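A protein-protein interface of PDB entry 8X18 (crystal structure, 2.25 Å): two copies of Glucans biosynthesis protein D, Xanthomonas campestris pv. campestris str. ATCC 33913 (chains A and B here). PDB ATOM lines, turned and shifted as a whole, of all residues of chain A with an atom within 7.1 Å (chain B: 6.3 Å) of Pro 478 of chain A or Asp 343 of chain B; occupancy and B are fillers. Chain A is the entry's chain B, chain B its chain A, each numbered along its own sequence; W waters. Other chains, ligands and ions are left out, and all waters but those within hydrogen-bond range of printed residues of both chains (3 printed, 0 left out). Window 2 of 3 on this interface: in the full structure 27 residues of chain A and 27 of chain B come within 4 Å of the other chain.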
ATOM      1  N   LEU A 449      15.785  22.461 -10.730  1.00  0.00           N
ATOM      2  CA  LEU A 449      14.578  22.574 -11.537  1.00  0.00           C
ATOM      3  C   LEU A 449      14.728  23.681 -12.583  1.00  0.00           C
ATOM      4  O   LEU A 449      14.155  23.547 -13.641  1.00  0.00           O
ATOM      5  CB  LEU A 449      13.351  22.847 -10.659  1.00  0.00           C
ATOM      6  CG  LEU A 449      12.829  21.666  -9.847  1.00  0.00           C
ATOM      7  CD1 LEU A 449      11.488  22.009  -9.224  1.00  0.00           C
ATOM      8  CD2 LEU A 449      12.684  20.435 -10.705  1.00  0.00           C
ATOM      9  N   LEU A 452      16.385  22.054 -15.515  1.00  0.00           N
ATOM     10  CA  LEU A 452      15.486  21.120 -16.181  1.00  0.00           C
ATOM     11  C   LEU A 452      14.365  21.841 -16.943  1.00  0.00           C
ATOM     12  O   LEU A 452      13.993  21.401 -18.023  1.00  0.00           O
ATOM     13  CB  LEU A 452      14.929  20.131 -15.157  1.00  0.00           C
ATOM     14  CG  LEU A 452      15.983  19.171 -14.609  1.00  0.00           C
ATOM     15  CD1 LEU A 452      15.456  18.361 -13.445  1.00  0.00           C
ATOM     16  CD2 LEU A 452      16.488  18.260 -15.720  1.00  0.00           C
ATOM     17  N   ALA A 453      13.814  22.928 -16.382  1.00  0.00           N
ATOM     18  CA  ALA A 453      12.725  23.658 -17.004  1.00  0.00           C
ATOM     19  C   ALA A 453      13.155  24.210 -18.366  1.00  0.00           C
ATOM     20  O   ALA A 453      12.362  24.236 -19.286  1.00  0.00           O
ATOM     21  CB  ALA A 453      12.275  24.770 -16.096  1.00  0.00           C
ATOM     22  N   LYS A 454      14.404  24.671 -18.483  1.00  0.00           N
ATOM     23  CA  LYS A 454      14.934  25.203 -19.737  1.00  0.00           C
ATOM     24  C   LYS A 454      15.334  24.090 -20.707  1.00  0.00           C
ATOM     25  O   LYS A 454      15.694  24.392 -21.828  1.00  0.00           O
ATOM     26  CB  LYS A 454      16.150  26.109 -19.483  1.00  0.00           C
ATOM     27  CG  LYS A 454      15.805  27.572 -19.236  1.00  0.00           C
ATOM     28  CD  LYS A 454      16.867  28.424 -18.533  1.00  0.00           C
ATOM     29  CE  LYS A 454      16.507  29.905 -18.527  1.00  0.00           C
ATOM     30  NZ  LYS A 454      16.672  30.537 -17.191  1.00  0.00           N
ATOM     31  N   ASP A 455      15.285  22.815 -20.312  1.00  0.00           N
ATOM     32  CA  ASP A 455      15.897  21.775 -21.121  1.00  0.00           C
ATOM     33  C   ASP A 455      14.798  20.958 -21.787  1.00  0.00           C
ATOM     34  O   ASP A 455      14.113  20.191 -21.120  1.00  0.00           O
ATOM     35  CB  ASP A 455      16.858  20.882 -20.324  1.00  0.00           C
ATOM     36  CG  ASP A 455      17.381  19.663 -21.086  1.00  0.00           C
ATOM     37  OD1 ASP A 455      17.078  19.546 -22.287  1.00  0.00           O
ATOM     38  OD2 ASP A 455      18.068  18.810 -20.466  1.00  0.00           O
ATOM     39  N   ALA A 458      14.390  17.214 -20.973  1.00  0.00           N
ATOM     40  CA  ALA A 458      14.291  16.831 -19.564  1.00  0.00           C
ATOM     41  C   ALA A 458      13.057  15.969 -19.302  1.00  0.00           C
ATOM     42  O   ALA A 458      11.961  16.339 -19.693  1.00  0.00           O
ATOM     43  CB  ALA A 458      14.243  18.085 -18.722  1.00  0.00           C
ATOM     44  N   VAL A 460      10.812  14.860 -16.397  1.00  0.00           N
ATOM     45  CA  VAL A 460      10.440  14.998 -15.003  1.00  0.00           C
ATOM     46  C   VAL A 460       9.080  14.347 -14.782  1.00  0.00           C
ATOM     47  O   VAL A 460       8.159  14.613 -15.533  1.00  0.00           O
ATOM     48  CB  VAL A 460      10.423  16.478 -14.598  1.00  0.00           C
ATOM     49  CG1 VAL A 460       9.845  16.694 -13.212  1.00  0.00           C
ATOM     50  CG2 VAL A 460      11.803  17.084 -14.691  1.00  0.00           C
ATOM     51  N   ALA A 476       3.224  16.952 -14.823  1.00  0.00           N
ATOM     52  CA  ALA A 476       4.320  17.684 -14.253  1.00  0.00           C
ATOM     53  C   ALA A 476       4.952  18.448 -15.399  1.00  0.00           C
ATOM     54  O   ALA A 476       5.419  17.813 -16.318  1.00  0.00           O
ATOM     55  CB  ALA A 476       5.303  16.729 -13.625  1.00  0.00           C
ATOM     56  N   ARG A 477       4.973  19.785 -15.336  1.00  0.00           N
ATOM     57  CA  ARG A 477       5.385  20.581 -16.479  1.00  0.00           C
ATOM     58  C   ARG A 477       6.161  21.780 -15.984  1.00  0.00           C
ATOM     59  O   ARG A 477       5.961  22.259 -14.870  1.00  0.00           O
ATOM     60  CB  ARG A 477       4.206  21.106 -17.313  1.00  0.00           C
ATOM     61  CG  ARG A 477       3.288  20.010 -17.834  1.00  0.00           C
ATOM     62  CD  ARG A 477       2.280  20.438 -18.886  1.00  0.00           C
ATOM     63  NE  ARG A 477       1.088  21.006 -18.265  1.00  0.00           N
ATOM     64  CZ  ARG A 477      -0.137  20.472 -18.291  1.00  0.00           C
ATOM     65  NH1 ARG A 477      -0.359  19.351 -18.963  1.00  0.00           N
ATOM     66  NH2 ARG A 477      -1.131  21.061 -17.634  1.00  0.00           N
ATOM     67  N   PRO A 478       7.061  22.315 -16.826  1.00  0.00           N
ATOM     68  CA  PRO A 478       7.778  23.520 -16.467  1.00  0.00           C
ATOM     69  C   PRO A 478       6.770  24.626 -16.158  1.00  0.00           C
ATOM     70  O   PRO A 478       5.725  24.725 -16.796  1.00  0.00           O
ATOM     71  CB  PRO A 478       8.626  23.806 -17.708  1.00  0.00           C
ATOM     72  CG  PRO A 478       8.702  22.494 -18.443  1.00  0.00           C
ATOM     73  CD  PRO A 478       7.409  21.793 -18.148  1.00  0.00           C
ATOM     74  N   LEU A 479       7.067  25.394 -15.114  1.00  0.00           N
ATOM     75  CA  LEU A 479       6.411  26.652 -14.856  1.00  0.00           C
ATOM     76  C   LEU A 479       7.452  27.740 -15.051  1.00  0.00           C
ATOM     77  O   LEU A 479       8.210  28.020 -14.116  1.00  0.00           O
ATOM     78  CB  LEU A 479       5.897  26.611 -13.414  1.00  0.00           C
ATOM     79  CG  LEU A 479       5.078  27.806 -12.952  1.00  0.00           C
ATOM     80  CD1 LEU A 479       3.909  28.083 -13.913  1.00  0.00           C
ATOM     81  CD2 LEU A 479       4.578  27.538 -11.543  1.00  0.00           C
ATOM     82  N   HIS A 480       7.589  28.230 -16.277  1.00  0.00           N
ATOM     83  CA  HIS A 480       8.706  29.153 -16.627  1.00  0.00           C
ATOM     84  C   HIS A 480       8.687  30.449 -15.815  1.00  0.00           C
ATOM     85  O   HIS A 480       9.761  30.984 -15.526  1.00  0.00           O
ATOM     86  CB  HIS A 480       8.689  29.375 -18.142  1.00  0.00           C
ATOM     87  CG  HIS A 480       8.858  28.114 -18.918  1.00  0.00           C
ATOM     88  ND1 HIS A 480      10.032  27.396 -18.920  1.00  0.00           N
ATOM     89  CD2 HIS A 480       8.013  27.441 -19.705  1.00  0.00           C
ATOM     90  CE1 HIS A 480       9.889  26.331 -19.691  1.00  0.00           C
ATOM     91  NE2 HIS A 480       8.671  26.340 -20.176  1.00  0.00           N
ATOM     92  N   GLU A 481       7.499  30.920 -15.462  1.00  0.00           N
ATOM     93  CA  GLU A 481       7.371  32.160 -14.699  1.00  0.00           C
ATOM     94  C   GLU A 481       8.050  32.011 -13.329  1.00  0.00           C
ATOM     95  O   GLU A 481       8.504  32.976 -12.731  1.00  0.00           O
ATOM     96  CB  GLU A 481       5.882  32.554 -14.539  1.00  0.00           C
ATOM     97  CG  GLU A 481       5.171  33.003 -15.842  1.00  0.00           C
ATOM     98  CD  GLU A 481       4.795  31.890 -16.817  1.00  0.00           C
ATOM     99  OE1 GLU A 481       4.942  30.646 -16.482  1.00  0.00           O
ATOM    100  OE2 GLU A 481       4.390  32.243 -17.933  1.00  0.00           O
ATOM    101  N   LYS A 483      10.633  29.588 -13.008  1.00  0.00           N
ATOM    102  CA  LYS A 483      11.804  28.747 -13.239  1.00  0.00           C
ATOM    103  C   LYS A 483      11.719  27.471 -12.406  1.00  0.00           C
ATOM    104  O   LYS A 483      12.694  26.988 -11.833  1.00  0.00           O
ATOM    105  CB  LYS A 483      13.072  29.571 -12.996  1.00  0.00           C
ATOM    106  CG  LYS A 483      13.276  30.632 -14.074  1.00  0.00           C
ATOM    107  CD  LYS A 483      14.333  31.682 -13.804  1.00  0.00           C
ATOM    108  CE  LYS A 483      14.433  32.662 -14.955  1.00  0.00           C
ATOM    109  NZ  LYS A 483      14.777  34.020 -14.478  1.00  0.00           N
ATOM    110  N   GLY A 484      10.553  26.832 -12.435  1.00  0.00           N
ATOM    111  CA  GLY A 484      10.373  25.604 -11.676  1.00  0.00           C
ATOM    112  C   GLY A 484       9.420  24.672 -12.396  1.00  0.00           C
ATOM    113  O   GLY A 484       9.326  24.735 -13.611  1.00  0.00           O
ATOM    114  N   TYR A 485       8.742  23.835 -11.622  1.00  0.00           N
ATOM    115  CA  TYR A 485       7.779  22.900 -12.151  1.00  0.00           C
ATOM    116  C   TYR A 485       6.467  22.997 -11.399  1.00  0.00           C
ATOM    117  O   TYR A 485       6.436  23.316 -10.205  1.00  0.00           O
ATOM    118  CB  TYR A 485       8.290  21.455 -12.083  1.00  0.00           C
ATOM    119  CG  TYR A 485       9.047  21.050 -13.328  1.00  0.00           C
ATOM    120  CD1 TYR A 485      10.278  21.611 -13.607  1.00  0.00           C
ATOM    121  CD2 TYR A 485       8.508  20.169 -14.248  1.00  0.00           C
ATOM    122  CE1 TYR A 485      10.978  21.249 -14.738  1.00  0.00           C
ATOM    123  CE2 TYR A 485       9.183  19.823 -15.409  1.00  0.00           C
ATOM    124  CZ  TYR A 485      10.427  20.361 -15.644  1.00  0.00           C
ATOM    125  OH  TYR A 485      11.141  20.052 -16.769  1.00  0.00           O
ATOM    126  N   ARG A 486       5.406  22.593 -12.114  1.00  0.00           N
ATOM    127  CA  ARG A 486       4.078  22.540 -11.544  1.00  0.00           C
ATOM    128  C   ARG A 486       3.554  21.140 -11.738  1.00  0.00           C
ATOM    129  O   ARG A 486       3.567  20.655 -12.869  1.00  0.00           O
ATOM    130  CB  ARG A 486       3.144  23.548 -12.219  1.00  0.00           C
ATOM    131  CG  ARG A 486       1.685  23.354 -11.836  1.00  0.00           C
ATOM    132  CD  ARG A 486       0.789  24.525 -12.162  1.00  0.00           C
ATOM    133  NE  ARG A 486       1.154  25.728 -11.420  1.00  0.00           N
ATOM    134  CZ  ARG A 486       0.807  26.972 -11.774  1.00  0.00           C
ATOM    135  NH1 ARG A 486       0.274  27.182 -12.969  1.00  0.00           N
ATOM    136  NH2 ARG A 486       1.083  28.002 -10.988  1.00  0.00           N
ATOM    137  N   MET A 488       0.070  18.875 -11.354  1.00  0.00           N
ATOM    138  CA  MET A 488      -1.370  18.970 -11.255  1.00  0.00           C
ATOM    139  C   MET A 488      -1.943  17.561 -11.206  1.00  0.00           C
ATOM    140  O   MET A 488      -1.445  16.654 -11.877  1.00  0.00           O
ATOM    141  CB  MET A 488      -1.934  19.760 -12.446  1.00  0.00           C
ATOM    142  CG  MET A 488      -1.695  21.257 -12.310  1.00  0.00           C
ATOM    143  SD  MET A 488      -2.398  22.203 -13.690  1.00  0.00           S
ATOM    144  CE  MET A 488      -4.100  22.155 -13.166  1.00  0.00           C
ATOM    145  N   TRP B 285      -8.794  26.508  -8.399  1.00  0.00           N
ATOM    146  CA  TRP B 285      -7.458  26.723  -7.854  1.00  0.00           C
ATOM    147  C   TRP B 285      -6.835  28.052  -8.312  1.00  0.00           C
ATOM    148  O   TRP B 285      -5.956  28.617  -7.631  1.00  0.00           O
ATOM    149  CB  TRP B 285      -6.549  25.537  -8.218  1.00  0.00           C
ATOM    150  CG  TRP B 285      -6.180  25.404  -9.666  1.00  0.00           C
ATOM    151  CD1 TRP B 285      -6.826  24.658 -10.611  1.00  0.00           C
ATOM    152  CD2 TRP B 285      -5.052  25.988 -10.336  1.00  0.00           C
ATOM    153  NE1 TRP B 285      -6.203  24.780 -11.833  1.00  0.00           N
ATOM    154  CE2 TRP B 285      -5.105  25.574 -11.691  1.00  0.00           C
ATOM    155  CE3 TRP B 285      -3.988  26.806  -9.918  1.00  0.00           C
ATOM    156  CZ2 TRP B 285      -4.156  25.962 -12.630  1.00  0.00           C
ATOM    157  CZ3 TRP B 285      -3.046  27.197 -10.854  1.00  0.00           C
ATOM    158  CH2 TRP B 285      -3.126  26.769 -12.186  1.00  0.00           C
ATOM    159  N   PHE B 337       0.857  38.177 -13.753  1.00  0.00           N
ATOM    160  CA  PHE B 337       0.626  36.753 -13.894  1.00  0.00           C
ATOM    161  C   PHE B 337       0.512  36.060 -12.536  1.00  0.00           C
ATOM    162  O   PHE B 337      -0.215  35.064 -12.393  1.00  0.00           O
ATOM    163  CB  PHE B 337       1.742  36.141 -14.742  1.00  0.00           C
ATOM    164  CG  PHE B 337       1.749  34.639 -14.724  1.00  0.00           C
ATOM    165  CD1 PHE B 337       2.372  33.941 -13.702  1.00  0.00           C
ATOM    166  CD2 PHE B 337       1.132  33.919 -15.728  1.00  0.00           C
ATOM    167  CE1 PHE B 337       2.371  32.554 -13.677  1.00  0.00           C
ATOM    168  CE2 PHE B 337       1.143  32.540 -15.705  1.00  0.00           C
ATOM    169  CZ  PHE B 337       1.769  31.857 -14.681  1.00  0.00           C
ATOM    170  N   GLN B 341      -2.067  32.787 -12.677  1.00  0.00           N
ATOM    171  CA  GLN B 341      -1.335  31.531 -12.602  1.00  0.00           C
ATOM    172  C   GLN B 341      -1.657  30.622 -13.781  1.00  0.00           C
ATOM    173  O   GLN B 341      -1.236  29.480 -13.780  1.00  0.00           O
ATOM    174  CB  GLN B 341      -1.522  30.804 -11.264  1.00  0.00           C
ATOM    175  CG  GLN B 341      -0.912  31.529 -10.069  1.00  0.00           C
ATOM    176  CD  GLN B 341       0.592  31.612 -10.135  1.00  0.00           C
ATOM    177  OE1 GLN B 341       1.274  30.843 -10.832  1.00  0.00           O
ATOM    178  NE2 GLN B 341       1.131  32.533  -9.356  1.00  0.00           N
ATOM    179  N   ASP B 342      -2.342  31.113 -14.820  1.00  0.00           N
ATOM    180  CA  ASP B 342      -2.707  30.223 -15.918  1.00  0.00           C
ATOM    181  C   ASP B 342      -1.715  30.389 -17.064  1.00  0.00           C
ATOM    182  O   ASP B 342      -1.819  31.319 -17.851  1.00  0.00           O
ATOM    183  CB  ASP B 342      -4.157  30.401 -16.363  1.00  0.00           C
ATOM    184  CG  ASP B 342      -4.634  29.271 -17.265  1.00  0.00           C
ATOM    185  OD1 ASP B 342      -3.859  28.910 -18.167  1.00  0.00           O
ATOM    186  OD2 ASP B 342      -5.787  28.812 -17.097  1.00  0.00           O
ATOM    187  N   ASP B 343      -0.739  29.482 -17.124  1.00  0.00           N
ATOM    188  CA  ASP B 343       0.307  29.570 -18.122  1.00  0.00           C
ATOM    189  C   ASP B 343      -0.138  28.804 -19.370  1.00  0.00           C
ATOM    190  O   ASP B 343       0.661  28.567 -20.245  1.00  0.00           O
ATOM    191  CB  ASP B 343       1.671  29.092 -17.587  1.00  0.00           C
ATOM    192  CG  ASP B 343       1.711  27.616 -17.189  1.00  0.00           C
ATOM    193  OD1 ASP B 343       0.657  27.040 -16.876  1.00  0.00           O
ATOM    194  OD2 ASP B 343       2.790  27.047 -17.228  1.00  0.00           O
ATOM    195  N   GLY B 344      -1.422  28.483 -19.467  1.00  0.00           N
ATOM    196  CA  GLY B 344      -2.041  27.997 -20.696  1.00  0.00           C
ATOM    197  C   GLY B 344      -2.762  29.099 -21.478  1.00  0.00           C
ATOM    198  O   GLY B 344      -2.509  29.200 -22.653  1.00  0.00           O
ATOM    199  N   VAL B 345      -3.569  29.969 -20.831  1.00  0.00           N
ATOM    200  CA  VAL B 345      -4.400  30.923 -21.564  1.00  0.00           C
ATOM    201  C   VAL B 345      -4.012  32.384 -21.344  1.00  0.00           C
ATOM    202  O   VAL B 345      -4.600  33.238 -21.984  1.00  0.00           O
ATOM    203  CB  VAL B 345      -5.906  30.727 -21.286  1.00  0.00           C
ATOM    204  CG1 VAL B 345      -6.338  29.335 -21.714  1.00  0.00           C
ATOM    205  CG2 VAL B 345      -6.274  30.985 -19.832  1.00  0.00           C
ATOM    206  N   PHE B 346      -3.079  32.656 -20.433  1.00  0.00           N
ATOM    207  CA  PHE B 346      -2.504  33.972 -20.179  1.00  0.00           C
ATOM    208  C   PHE B 346      -3.558  35.060 -20.039  1.00  0.00           C
ATOM    209  O   PHE B 346      -3.584  36.011 -20.812  1.00  0.00           O
ATOM    210  CB  PHE B 346      -1.485  34.286 -21.274  1.00  0.00           C
ATOM    211  CG  PHE B 346      -0.349  33.284 -21.296  1.00  0.00           C
ATOM    212  CD1 PHE B 346       0.653  33.325 -20.334  1.00  0.00           C
ATOM    213  CD2 PHE B 346      -0.305  32.257 -22.241  1.00  0.00           C
ATOM    214  CE1 PHE B 346       1.692  32.396 -20.328  1.00  0.00           C
ATOM    215  CE2 PHE B 346       0.732  31.325 -22.227  1.00  0.00           C
ATOM    216  CZ  PHE B 346       1.724  31.394 -21.273  1.00  0.00           C
HETATM  217  O   HOH W   1       4.989  28.446 -17.566  1.00  0.00           O
HETATM  218  O   HOH W   2       3.063  24.625 -15.881  1.00  0.00           O
HETATM  219  O   HOH W   3      -0.575  25.424 -15.277  1.00  0.00           O
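The guanidinium group of Arg 486 of chain A lies within salt-bridge range of the side-chain carboxylate of Asp 343 of chain B. NH2 of Arg 486 of chain A lies within hydrogen-bond range of OE1 of Gln 341 of chain B, 2.9 Å away.
O of Gly 484 of chain A lies within hydrogen-bond range of N of Leu 479 of chain A (2.8 Å). The backbone carbonyl oxygen (O) of Arg 477 of chain A sits at hydrogen-bond distance from the backbone NH (N) of Arg 486 of chain A (2.8 Å).
Among the printed residues, pairs that only touch across the chains: Pro 478 of chain A with Asp 343 of chain B, Leu 479 of chain A with Asp 343 of chain B, Glu 481 of chain A with Phe 337 of chain B, Glu 481 of chain A with Asp 343 of chain B, Glu 481 of chain A with Phe 346 of chain B, Arg 486 of chain A with Trp 285 of chain B and Met 488 of chain A with Trp 285 of chain B.
Pro 478 of chain A touches one residue of chain B. Asp 343 of chain B touches four residues of chain A. Printed residues of chain A within 4 Å of Trp 285 of chain B: Arg 486 (3.5 Å) and Met 488 (3.6 Å). Of the printed residues of chain B, Leu 479 of chain A touches Asp 343. Printed residues of chain A within 4 Å of Gln 341 of chain B: Arg 486 (2.9 Å). Of the printed residues of chain B, Glu 481 of chain A touches Phe 337, Asp 343 and Phe 346. Val 460 of chain A touches none of the printed residues of chain B. Val 345 of chain B touches none of the printed residues of chain A. The nearest printed residue of chain B that does not touch Pro 478 of chain A is Phe 337 of chain B (8.4 Å). The nearest residue of chain A that does not touch Asp 343 of chain B is His 480 of chain A (5.0 Å). The nearest printed residue of chain B that does not touch Glu 481 of chain A is Gln 341 of chain B (6.2 Å).
Hydrophobic or aromatic side chains of chain B within 4 Å of the printed part of chain A: Trp 285, Phe 337 and Phe 346. Hydrophobic or aromatic side chains of chain A that line the printed part of chain B: Leu 479 and Met 488. Among the printed residues, 9 pairs touch across the chains.
No position is printed for both chains. Of the 9 pairs that touch across the chains among the printed residues, none has its exchanged pair printed and touching as well.
Water W1 lies within hydrogen-bond range of OE1 of Glu 481 of chain A, OD2 of Asp 343 of chain B and N of His 480 of chain A. Water W3 bridges the side-chain carboxylate of Asp 343 of chain B (2.6 Å) and the guanidinium group of Arg 486 of chain A (3.0 Å). Water W2 bridges OD2 of Asp 343 of chain B (2.8 Å) and O of Pro 478 of chain A (2.8 Å).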
